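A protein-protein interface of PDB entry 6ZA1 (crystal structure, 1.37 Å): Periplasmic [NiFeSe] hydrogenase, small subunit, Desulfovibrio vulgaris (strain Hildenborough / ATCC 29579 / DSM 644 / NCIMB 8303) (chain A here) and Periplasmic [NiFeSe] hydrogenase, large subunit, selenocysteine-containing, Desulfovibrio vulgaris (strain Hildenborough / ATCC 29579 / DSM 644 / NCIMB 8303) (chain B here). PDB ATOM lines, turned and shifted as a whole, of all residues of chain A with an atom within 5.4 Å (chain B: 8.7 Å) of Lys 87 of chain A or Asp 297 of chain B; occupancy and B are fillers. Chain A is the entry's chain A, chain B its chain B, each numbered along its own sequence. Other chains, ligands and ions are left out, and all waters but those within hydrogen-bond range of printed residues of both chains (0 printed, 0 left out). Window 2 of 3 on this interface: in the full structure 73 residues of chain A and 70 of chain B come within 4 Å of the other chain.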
ATOM      1  N   PRO A  81       2.561  15.163  -5.745  1.00  0.00           N
ATOM      2  CA  PRO A  81       3.507  14.127  -5.306  1.00  0.00           C
ATOM      3  C   PRO A  81       4.073  13.343  -6.477  1.00  0.00           C
ATOM      4  O   PRO A  81       3.317  12.798  -7.288  1.00  0.00           O
ATOM      5  CB  PRO A  81       2.653  13.239  -4.397  1.00  0.00           C
ATOM      6  CG  PRO A  81       1.275  13.308  -5.033  1.00  0.00           C
ATOM      7  CD  PRO A  81       1.156  14.713  -5.628  1.00  0.00           C
ATOM      8  N   GLU A  83       6.550  10.782  -6.202  1.00  0.00           N
ATOM      9  CA  GLU A  83       7.015   9.435  -5.916  1.00  0.00           C
ATOM     10  C   GLU A  83       6.022   8.397  -6.435  1.00  0.00           C
ATOM     11  O   GLU A  83       4.849   8.685  -6.691  1.00  0.00           O
ATOM     12  CB  GLU A  83       7.189   9.229  -4.413  1.00  0.00           C
ATOM     13  CG  GLU A  83       8.420   9.891  -3.829  1.00  0.00           C
ATOM     14  CD  GLU A  83       9.711   9.275  -4.331  1.00  0.00           C
ATOM     15  OE1 GLU A  83       9.710   8.082  -4.705  1.00  0.00           O
ATOM     16  OE2 GLU A  83      10.733   9.990  -4.349  1.00  0.00           O
ATOM     17  N   ALA A  84       6.514   7.166  -6.574  1.00  0.00           N
ATOM     18  CA  ALA A  84       5.687   6.041  -7.002  1.00  0.00           C
ATOM     19  C   ALA A  84       4.952   6.362  -8.298  1.00  0.00           C
ATOM     20  O   ALA A  84       3.772   6.053  -8.460  1.00  0.00           O
ATOM     21  CB  ALA A  84       4.711   5.623  -5.901  1.00  0.00           C
ATOM     22  N   ASP A  85       5.656   7.012  -9.225  1.00  0.00           N
ATOM     23  CA  ASP A  85       5.113   7.317 -10.548  1.00  0.00           C
ATOM     24  C   ASP A  85       3.808   8.104 -10.466  1.00  0.00           C
ATOM     25  O   ASP A  85       2.911   7.923 -11.294  1.00  0.00           O
ATOM     26  CB  ASP A  85       4.921   6.038 -11.373  1.00  0.00           C
ATOM     27  CG  ASP A  85       4.876   6.304 -12.862  1.00  0.00           C
ATOM     28  OD1 ASP A  85       5.023   7.477 -13.262  1.00  0.00           O
ATOM     29  OD2 ASP A  85       4.701   5.337 -13.634  1.00  0.00           O
ATOM     30  N   GLY A  86       3.682   8.970  -9.458  1.00  0.00           N
ATOM     31  CA  GLY A  86       2.516   9.814  -9.294  1.00  0.00           C
ATOM     32  C   GLY A  86       1.349   9.191  -8.561  1.00  0.00           C
ATOM     33  O   GLY A  86       0.321   9.858  -8.392  1.00  0.00           O
ATOM     34  N   LYS A  87       1.485   7.950  -8.090  1.00  0.00           N
ATOM     35  CA  LYS A  87       0.344   7.185  -7.603  1.00  0.00           C
ATOM     36  C   LYS A  87      -0.199   7.675  -6.268  1.00  0.00           C
ATOM     37  O   LYS A  87      -1.276   7.220  -5.857  1.00  0.00           O
ATOM     38  CB  LYS A  87       0.738   5.712  -7.466  1.00  0.00           C
ATOM     39  CG  LYS A  87       0.949   4.961  -8.770  1.00  0.00           C
ATOM     40  CD  LYS A  87       1.297   3.502  -8.490  1.00  0.00           C
ATOM     41  CE  LYS A  87       1.257   2.638  -9.746  1.00  0.00           C
ATOM     42  NZ  LYS A  87       1.410   1.187  -9.428  1.00  0.00           N
ATOM     43  N   TYR A  88       0.497   8.566  -5.571  1.00  0.00           N
ATOM     44  CA  TYR A  88      -0.033   9.099  -4.325  1.00  0.00           C
ATOM     45  C   TYR A  88      -1.108  10.157  -4.531  1.00  0.00           C
ATOM     46  O   TYR A  88      -1.669  10.643  -3.544  1.00  0.00           O
ATOM     47  CB  TYR A  88       1.094   9.645  -3.443  1.00  0.00           C
ATOM     48  CG  TYR A  88       1.962   8.568  -2.830  1.00  0.00           C
ATOM     49  CD1 TYR A  88       1.420   7.596  -1.996  1.00  0.00           C
ATOM     50  CD2 TYR A  88       3.329   8.531  -3.070  1.00  0.00           C
ATOM     51  CE1 TYR A  88       2.213   6.608  -1.430  1.00  0.00           C
ATOM     52  CE2 TYR A  88       4.131   7.552  -2.505  1.00  0.00           C
ATOM     53  CZ  TYR A  88       3.567   6.593  -1.686  1.00  0.00           C
ATOM     54  OH  TYR A  88       4.358   5.614  -1.123  1.00  0.00           O
ATOM     55  N   CYS A  89      -1.428  10.522  -5.779  1.00  0.00           N
ATOM     56  CA  CYS A  89      -2.572  11.409  -6.023  1.00  0.00           C
ATOM     57  C   CYS A  89      -3.170  11.101  -7.395  1.00  0.00           C
ATOM     58  O   CYS A  89      -2.669  11.585  -8.413  1.00  0.00           O
ATOM     59  CB  CYS A  89      -2.174  12.871  -5.923  1.00  0.00           C
ATOM     60  SG  CYS A  89      -3.594  13.972  -6.017  1.00  0.00           S
ATOM     61  N   ILE A  90      -4.263  10.339  -7.410  1.00  0.00           N
ATOM     62  CA  ILE A  90      -5.033  10.074  -8.622  1.00  0.00           C
ATOM     63  C   ILE A  90      -6.269  10.962  -8.598  1.00  0.00           C
ATOM     64  O   ILE A  90      -7.054  10.913  -7.640  1.00  0.00           O
ATOM     65  CB  ILE A  90      -5.428   8.593  -8.720  1.00  0.00           C
ATOM     66  CG1 ILE A  90      -4.183   7.699  -8.733  1.00  0.00           C
ATOM     67  CG2 ILE A  90      -6.294   8.353  -9.959  1.00  0.00           C
ATOM     68  CD1 ILE A  90      -3.161   8.039  -9.805  1.00  0.00           C
ATOM     69  N   SER A 100      -3.037  10.809 -12.866  1.00  0.00           N
ATOM     70  CA  SER A 100      -2.424  11.326 -11.648  1.00  0.00           C
ATOM     71  C   SER A 100      -2.355  12.850 -11.694  1.00  0.00           C
ATOM     72  O   SER A 100      -2.547  13.476 -12.743  1.00  0.00           O
ATOM     73  CB  SER A 100      -1.007  10.781 -11.484  1.00  0.00           C
ATOM     74  OG  SER A 100      -0.153  11.258 -12.511  1.00  0.00           O
ATOM     75  N   SER B  37     -12.316   3.513  -3.826  1.00  0.00           N
ATOM     76  CA  SER B  37     -10.874   3.717  -3.823  1.00  0.00           C
ATOM     77  C   SER B  37     -10.563   5.161  -3.468  1.00  0.00           C
ATOM     78  O   SER B  37     -10.918   6.078  -4.218  1.00  0.00           O
ATOM     79  CB  SER B  37     -10.288   3.376  -5.194  1.00  0.00           C
ATOM     80  OG  SER B  37      -8.907   3.681  -5.236  1.00  0.00           O
ATOM     81  N   GLY B  38      -9.897   5.357  -2.338  1.00  0.00           N
ATOM     82  CA  GLY B  38      -9.379   6.667  -2.000  1.00  0.00           C
ATOM     83  C   GLY B  38      -8.009   6.832  -2.616  1.00  0.00           C
ATOM     84  O   GLY B  38      -7.084   6.078  -2.303  1.00  0.00           O
ATOM     85  N   GLY B  39      -7.866   7.812  -3.504  1.00  0.00           N
ATOM     86  CA  GLY B  39      -6.722   7.886  -4.382  1.00  0.00           C
ATOM     87  C   GLY B  39      -5.650   8.898  -4.048  1.00  0.00           C
ATOM     88  O   GLY B  39      -4.743   9.095  -4.864  1.00  0.00           O
ATOM     89  N   MET B  40      -5.712   9.550  -2.890  1.00  0.00           N
ATOM     90  CA  MET B  40      -4.705  10.539  -2.525  1.00  0.00           C
ATOM     91  C   MET B  40      -4.239  10.317  -1.096  1.00  0.00           C
ATOM     92  O   MET B  40      -5.056  10.181  -0.181  1.00  0.00           O
ATOM     93  CB  MET B  40      -5.226  11.971  -2.695  1.00  0.00           C
ATOM     94  CG  MET B  40      -4.157  13.039  -2.473  1.00  0.00           C
ATOM     95  SD  MET B  40      -3.934  13.525  -0.752  1.00  0.00           S
ATOM     96  CE  MET B  40      -5.345  14.597  -0.547  1.00  0.00           C
ATOM     97  N   TYR B  41      -2.917  10.304  -0.913  1.00  0.00           N
ATOM     98  CA  TYR B  41      -2.288  10.044   0.374  1.00  0.00           C
ATOM     99  C   TYR B  41      -1.276  11.133   0.699  1.00  0.00           C
ATOM    100  O   TYR B  41      -0.536  11.587  -0.176  1.00  0.00           O
ATOM    101  CB  TYR B  41      -1.562   8.684   0.323  1.00  0.00           C
ATOM    102  CG  TYR B  41      -0.731   8.336   1.537  1.00  0.00           C
ATOM    103  CD1 TYR B  41      -1.320   7.783   2.660  1.00  0.00           C
ATOM    104  CD2 TYR B  41       0.645   8.544   1.553  1.00  0.00           C
ATOM    105  CE1 TYR B  41      -0.573   7.451   3.776  1.00  0.00           C
ATOM    106  CE2 TYR B  41       1.405   8.217   2.670  1.00  0.00           C
ATOM    107  CZ  TYR B  41       0.786   7.666   3.779  1.00  0.00           C
ATOM    108  OH  TYR B  41       1.510   7.329   4.903  1.00  0.00           O
ATOM    109  N   SER B 276      -5.692  -2.463   1.052  1.00  0.00           N
ATOM    110  CA  SER B 276      -5.240  -1.085   1.156  1.00  0.00           C
ATOM    111  C   SER B 276      -3.756  -1.022   0.831  1.00  0.00           C
ATOM    112  O   SER B 276      -3.014  -1.990   1.044  1.00  0.00           O
ATOM    113  CB  SER B 276      -5.458  -0.564   2.578  1.00  0.00           C
ATOM    114  OG  SER B 276      -6.788  -0.790   3.013  1.00  0.00           O
ATOM    115  N   TRP B 277      -3.318   0.128   0.328  1.00  0.00           N
ATOM    116  CA  TRP B 277      -1.940   0.279  -0.137  1.00  0.00           C
ATOM    117  C   TRP B 277      -0.983   0.554   1.030  1.00  0.00           C
ATOM    118  O   TRP B 277      -0.347   1.603   1.128  1.00  0.00           O
ATOM    119  CB  TRP B 277      -1.861   1.357  -1.207  1.00  0.00           C
ATOM    120  CG  TRP B 277      -2.422   0.946  -2.529  1.00  0.00           C
ATOM    121  CD1 TRP B 277      -2.090  -0.159  -3.261  1.00  0.00           C
ATOM    122  CD2 TRP B 277      -3.401   1.652  -3.291  1.00  0.00           C
ATOM    123  NE1 TRP B 277      -2.809  -0.182  -4.433  1.00  0.00           N
ATOM    124  CE2 TRP B 277      -3.623   0.921  -4.473  1.00  0.00           C
ATOM    125  CE3 TRP B 277      -4.116   2.838  -3.087  1.00  0.00           C
ATOM    126  CZ2 TRP B 277      -4.530   1.333  -5.448  1.00  0.00           C
ATOM    127  CZ3 TRP B 277      -5.016   3.244  -4.056  1.00  0.00           C
ATOM    128  CH2 TRP B 277      -5.214   2.493  -5.222  1.00  0.00           C
ATOM    129  N   PHE B 278      -0.888  -0.437   1.916  1.00  0.00           N
ATOM    130  CA  PHE B 278       0.008  -0.404   3.064  1.00  0.00           C
ATOM    131  C   PHE B 278       0.655  -1.767   3.212  1.00  0.00           C
ATOM    132  O   PHE B 278       0.134  -2.780   2.740  1.00  0.00           O
ATOM    133  CB  PHE B 278      -0.732   0.008   4.347  1.00  0.00           C
ATOM    134  CG  PHE B 278      -1.318   1.373   4.245  1.00  0.00           C
ATOM    135  CD1 PHE B 278      -0.517   2.480   4.432  1.00  0.00           C
ATOM    136  CD2 PHE B 278      -2.640   1.557   3.877  1.00  0.00           C
ATOM    137  CE1 PHE B 278      -1.024   3.749   4.290  1.00  0.00           C
ATOM    138  CE2 PHE B 278      -3.159   2.833   3.735  1.00  0.00           C
ATOM    139  CZ  PHE B 278      -2.346   3.931   3.939  1.00  0.00           C
ATOM    140  N   ALA B 279       1.803  -1.784   3.881  1.00  0.00           N
ATOM    141  CA  ALA B 279       2.562  -3.015   4.022  1.00  0.00           C
ATOM    142  C   ALA B 279       1.747  -4.099   4.720  1.00  0.00           C
ATOM    143  O   ALA B 279       1.101  -3.861   5.745  1.00  0.00           O
ATOM    144  CB  ALA B 279       3.842  -2.740   4.809  1.00  0.00           C
ATOM    145  N   PRO B 294       3.242   3.051   3.726  1.00  0.00           N
ATOM    146  CA  PRO B 294       2.584   2.989   2.415  1.00  0.00           C
ATOM    147  C   PRO B 294       3.222   1.949   1.504  1.00  0.00           C
ATOM    148  O   PRO B 294       4.432   1.721   1.536  1.00  0.00           O
ATOM    149  CB  PRO B 294       2.736   4.415   1.864  1.00  0.00           C
ATOM    150  CG  PRO B 294       3.892   5.008   2.618  1.00  0.00           C
ATOM    151  CD  PRO B 294       3.877   4.361   3.979  1.00  0.00           C
ATOM    152  N   ALA B 295       2.382   1.310   0.692  1.00  0.00           N
ATOM    153  CA  ALA B 295       2.819   0.313  -0.287  1.00  0.00           C
ATOM    154  C   ALA B 295       1.953   0.482  -1.526  1.00  0.00           C
ATOM    155  O   ALA B 295       1.056  -0.325  -1.796  1.00  0.00           O
ATOM    156  CB  ALA B 295       2.698  -1.097   0.288  1.00  0.00           C
ATOM    157  N   PRO B 296       2.201   1.536  -2.316  1.00  0.00           N
ATOM    158  CA  PRO B 296       1.300   1.839  -3.440  1.00  0.00           C
ATOM    159  C   PRO B 296       1.373   0.844  -4.587  1.00  0.00           C
ATOM    160  O   PRO B 296       0.535   0.918  -5.495  1.00  0.00           O
ATOM    161  CB  PRO B 296       1.749   3.234  -3.894  1.00  0.00           C
ATOM    162  CG  PRO B 296       3.207   3.282  -3.527  1.00  0.00           C
ATOM    163  CD  PRO B 296       3.325   2.493  -2.232  1.00  0.00           C
ATOM    164  N   ASP B 297       2.338  -0.064  -4.594  1.00  0.00           N
ATOM    165  CA  ASP B 297       2.431  -1.065  -5.644  1.00  0.00           C
ATOM    166  C   ASP B 297       1.962  -2.441  -5.183  1.00  0.00           C
ATOM    167  O   ASP B 297       2.203  -3.428  -5.885  1.00  0.00           O
ATOM    168  CB  ASP B 297       3.859  -1.107  -6.202  1.00  0.00           C
ATOM    169  CG  ASP B 297       4.281   0.227  -6.819  1.00  0.00           C
ATOM    170  OD1 ASP B 297       3.479   0.817  -7.577  1.00  0.00           O
ATOM    171  OD2 ASP B 297       5.404   0.695  -6.535  1.00  0.00           O
ATOM    172  N   LYS B 298       1.261  -2.529  -4.049  1.00  0.00           N
ATOM    173  CA  LYS B 298       0.883  -3.838  -3.525  1.00  0.00           C
ATOM    174  C   LYS B 298      -0.238  -4.455  -4.353  1.00  0.00           C
ATOM    175  O   LYS B 298      -1.319  -3.869  -4.489  1.00  0.00           O
ATOM    176  CB  LYS B 298       0.454  -3.767  -2.061  1.00  0.00           C
ATOM    177  CG  LYS B 298       0.192  -5.171  -1.500  1.00  0.00           C
ATOM    178  CD  LYS B 298      -0.107  -5.173  -0.019  1.00  0.00           C
ATOM    179  CE  LYS B 298      -1.478  -4.589   0.265  1.00  0.00           C
ATOM    180  NZ  LYS B 298      -1.755  -4.563   1.725  1.00  0.00           N
ATOM    181  N   ALA B 299       0.005  -5.665  -4.856  1.00  0.00           N
ATOM    182  CA  ALA B 299      -0.969  -6.343  -5.699  1.00  0.00           C
ATOM    183  C   ALA B 299      -2.267  -6.581  -4.942  1.00  0.00           C
ATOM    184  O   ALA B 299      -2.267  -6.996  -3.779  1.00  0.00           O
ATOM    185  CB  ALA B 299      -0.397  -7.683  -6.169  1.00  0.00           C
ATOM    186  N   GLY B 300      -3.384  -6.315  -5.616  1.00  0.00           N
ATOM    187  CA  GLY B 300      -4.693  -6.611  -5.091  1.00  0.00           C
ATOM    188  C   GLY B 300      -5.324  -5.509  -4.273  1.00  0.00           C
ATOM    189  O   GLY B 300      -6.549  -5.513  -4.101  1.00  0.00           O
ATOM    190  N   ALA B 301      -4.533  -4.573  -3.761  1.00  0.00           N
ATOM    191  CA  ALA B 301      -5.077  -3.474  -2.982  1.00  0.00           C
ATOM    192  C   ALA B 301      -5.668  -2.414  -3.905  1.00  0.00           C
ATOM    193  O   ALA B 301      -5.289  -2.299  -5.077  1.00  0.00           O
ATOM    194  CB  ALA B 301      -3.995  -2.855  -2.098  1.00  0.00           C
ATOM    195  N   SER B 303      -7.007   0.976  -2.413  1.00  0.00           N
ATOM    196  CA  SER B 303      -7.352   2.221  -1.744  1.00  0.00           C
ATOM    197  C   SER B 303      -6.261   2.604  -0.759  1.00  0.00           C
ATOM    198  O   SER B 303      -5.569   1.743  -0.219  1.00  0.00           O
ATOM    199  CB  SER B 303      -8.685   2.071  -1.002  1.00  0.00           C
ATOM    200  OG  SER B 303      -9.092   3.288  -0.411  1.00  0.00           O
ATOM    201  N   PHE B 304      -6.117   3.911  -0.531  1.00  0.00           N
ATOM    202  CA  PHE B 304      -5.278   4.415   0.547  1.00  0.00           C
ATOM    203  C   PHE B 304      -6.021   4.499   1.882  1.00  0.00           C
ATOM    204  O   PHE B 304      -5.422   4.907   2.887  1.00  0.00           O
ATOM    205  CB  PHE B 304      -4.692   5.786   0.178  1.00  0.00           C
ATOM    206  CG  PHE B 304      -3.574   5.726  -0.840  1.00  0.00           C
ATOM    207  CD1 PHE B 304      -2.382   5.079  -0.547  1.00  0.00           C
ATOM    208  CD2 PHE B 304      -3.707   6.340  -2.080  1.00  0.00           C
ATOM    209  CE1 PHE B 304      -1.351   5.032  -1.469  1.00  0.00           C
ATOM    210  CE2 PHE B 304      -2.674   6.297  -3.006  1.00  0.00           C
ATOM    211  CZ  PHE B 304      -1.495   5.643  -2.699  1.00  0.00           C
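The backbone carbonyl oxygen (O) of Gly 38 of chain B sits at hydrogen-bond distance from the backbone NH (N) of Phe 304 of chain B, at 3.0 Å.
Of the 19 printed residues of chain B, 7 touch a printed residue of chain A.
Hydrophobic or aromatic side chains of chain B within 4 Å of the printed part of chain A: Met 40, Tyr 41, Pro 294, Pro 296 and Phe 304.
Printed residues of chain A that touch a printed residue of chain B: Ala 84, Lys 87, Tyr 88, Cys 89 and Ile 90.
Among the printed residues, 12 pairs touch across the chains.
Among the printed residues, Asp or Glu carboxylates within 4 Å of a Lys or Arg side-chain nitrogen of the other chain: Lys 87 of chain A with Asp 297 of chain B.
Among the printed residues, pairs that only touch across the chains: Ala 84 of chain A with Pro 296 of chain B (3.7 Å), Lys 87 of chain A with Phe 304 of chain B (3.3 Å), Tyr 88 of chain A with Gly 39 of chain B (3.7 Å), Tyr 88 of chain A with Met 40 of chain B (3.2 Å), Tyr 88 of chain A with Pro 294 of chain B (3.6 Å), Tyr 88 of chain A with Pro 296 of chain B (3.5 Å), Tyr 88 of chain A with Phe 304 of chain B (3.6 Å), Cys 89 of chain A with Gly 39 of chain B (3.4 Å) and Cys 89 of chain A with Met 40 of chain B (3.7 Å).
Of the printed residues of chain B, Lys 87 of chain A touches Asp 297 and Phe 304.
Of chain A, only Lys 87 (2.8 Å) comes within 4 Å of Asp 297 of chain B.
No residue of chain B comes within 4 Å of Gly 86 of chain A.
Of the printed residues of chain B, Cys 89 of chain A touches Gly 39 and Met 40.
Printed residues of chain A within 4 Å of Tyr 41 of chain B: Tyr 88 (2.9 Å).
Printed residues of chain A within 4 Å of Phe 304 of chain B: Lys 87 (3.3 Å) and Tyr 88 (3.6 Å).
Printed residues of chain B within 4 Å of Tyr 88 of chain A: Gly 39 (3.7 Å), Met 40 (3.2 Å), Tyr 41 (2.9 Å), Pro 294 (3.6 Å), Pro 296 (3.5 Å) and Phe 304 (3.6 Å).
Of the printed residues of chain A, Gly 39 of chain B touches Tyr 88, Cys 89 and Ile 90.
Ala 295 of chain B touches none of the printed residues of chain A.
Ser 100 of chain A touches none of the printed residues of chain B.
The nearest residue of chain B that does not touch Lys 87 of chain A is Pro 296 of chain B (4.03 Å).
The side-chain amino group (NZ) of Lys 87 of chain A lies within salt-bridge range of the side-chain carboxylate (OD1) of Asp 297 of chain B (2.8 Å).
The backbone NH (N) of Tyr 41 of chain B lies within hydrogen-bond range of the backbone carbonyl oxygen (O) of Tyr 88 of chain A, at 2.9 Å.
The backbone NH of Ile 90 of chain A lies within hydrogen-bond range of the backbone carbonyl oxygen of Gly 39 of chain B, 2.9 Å away.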
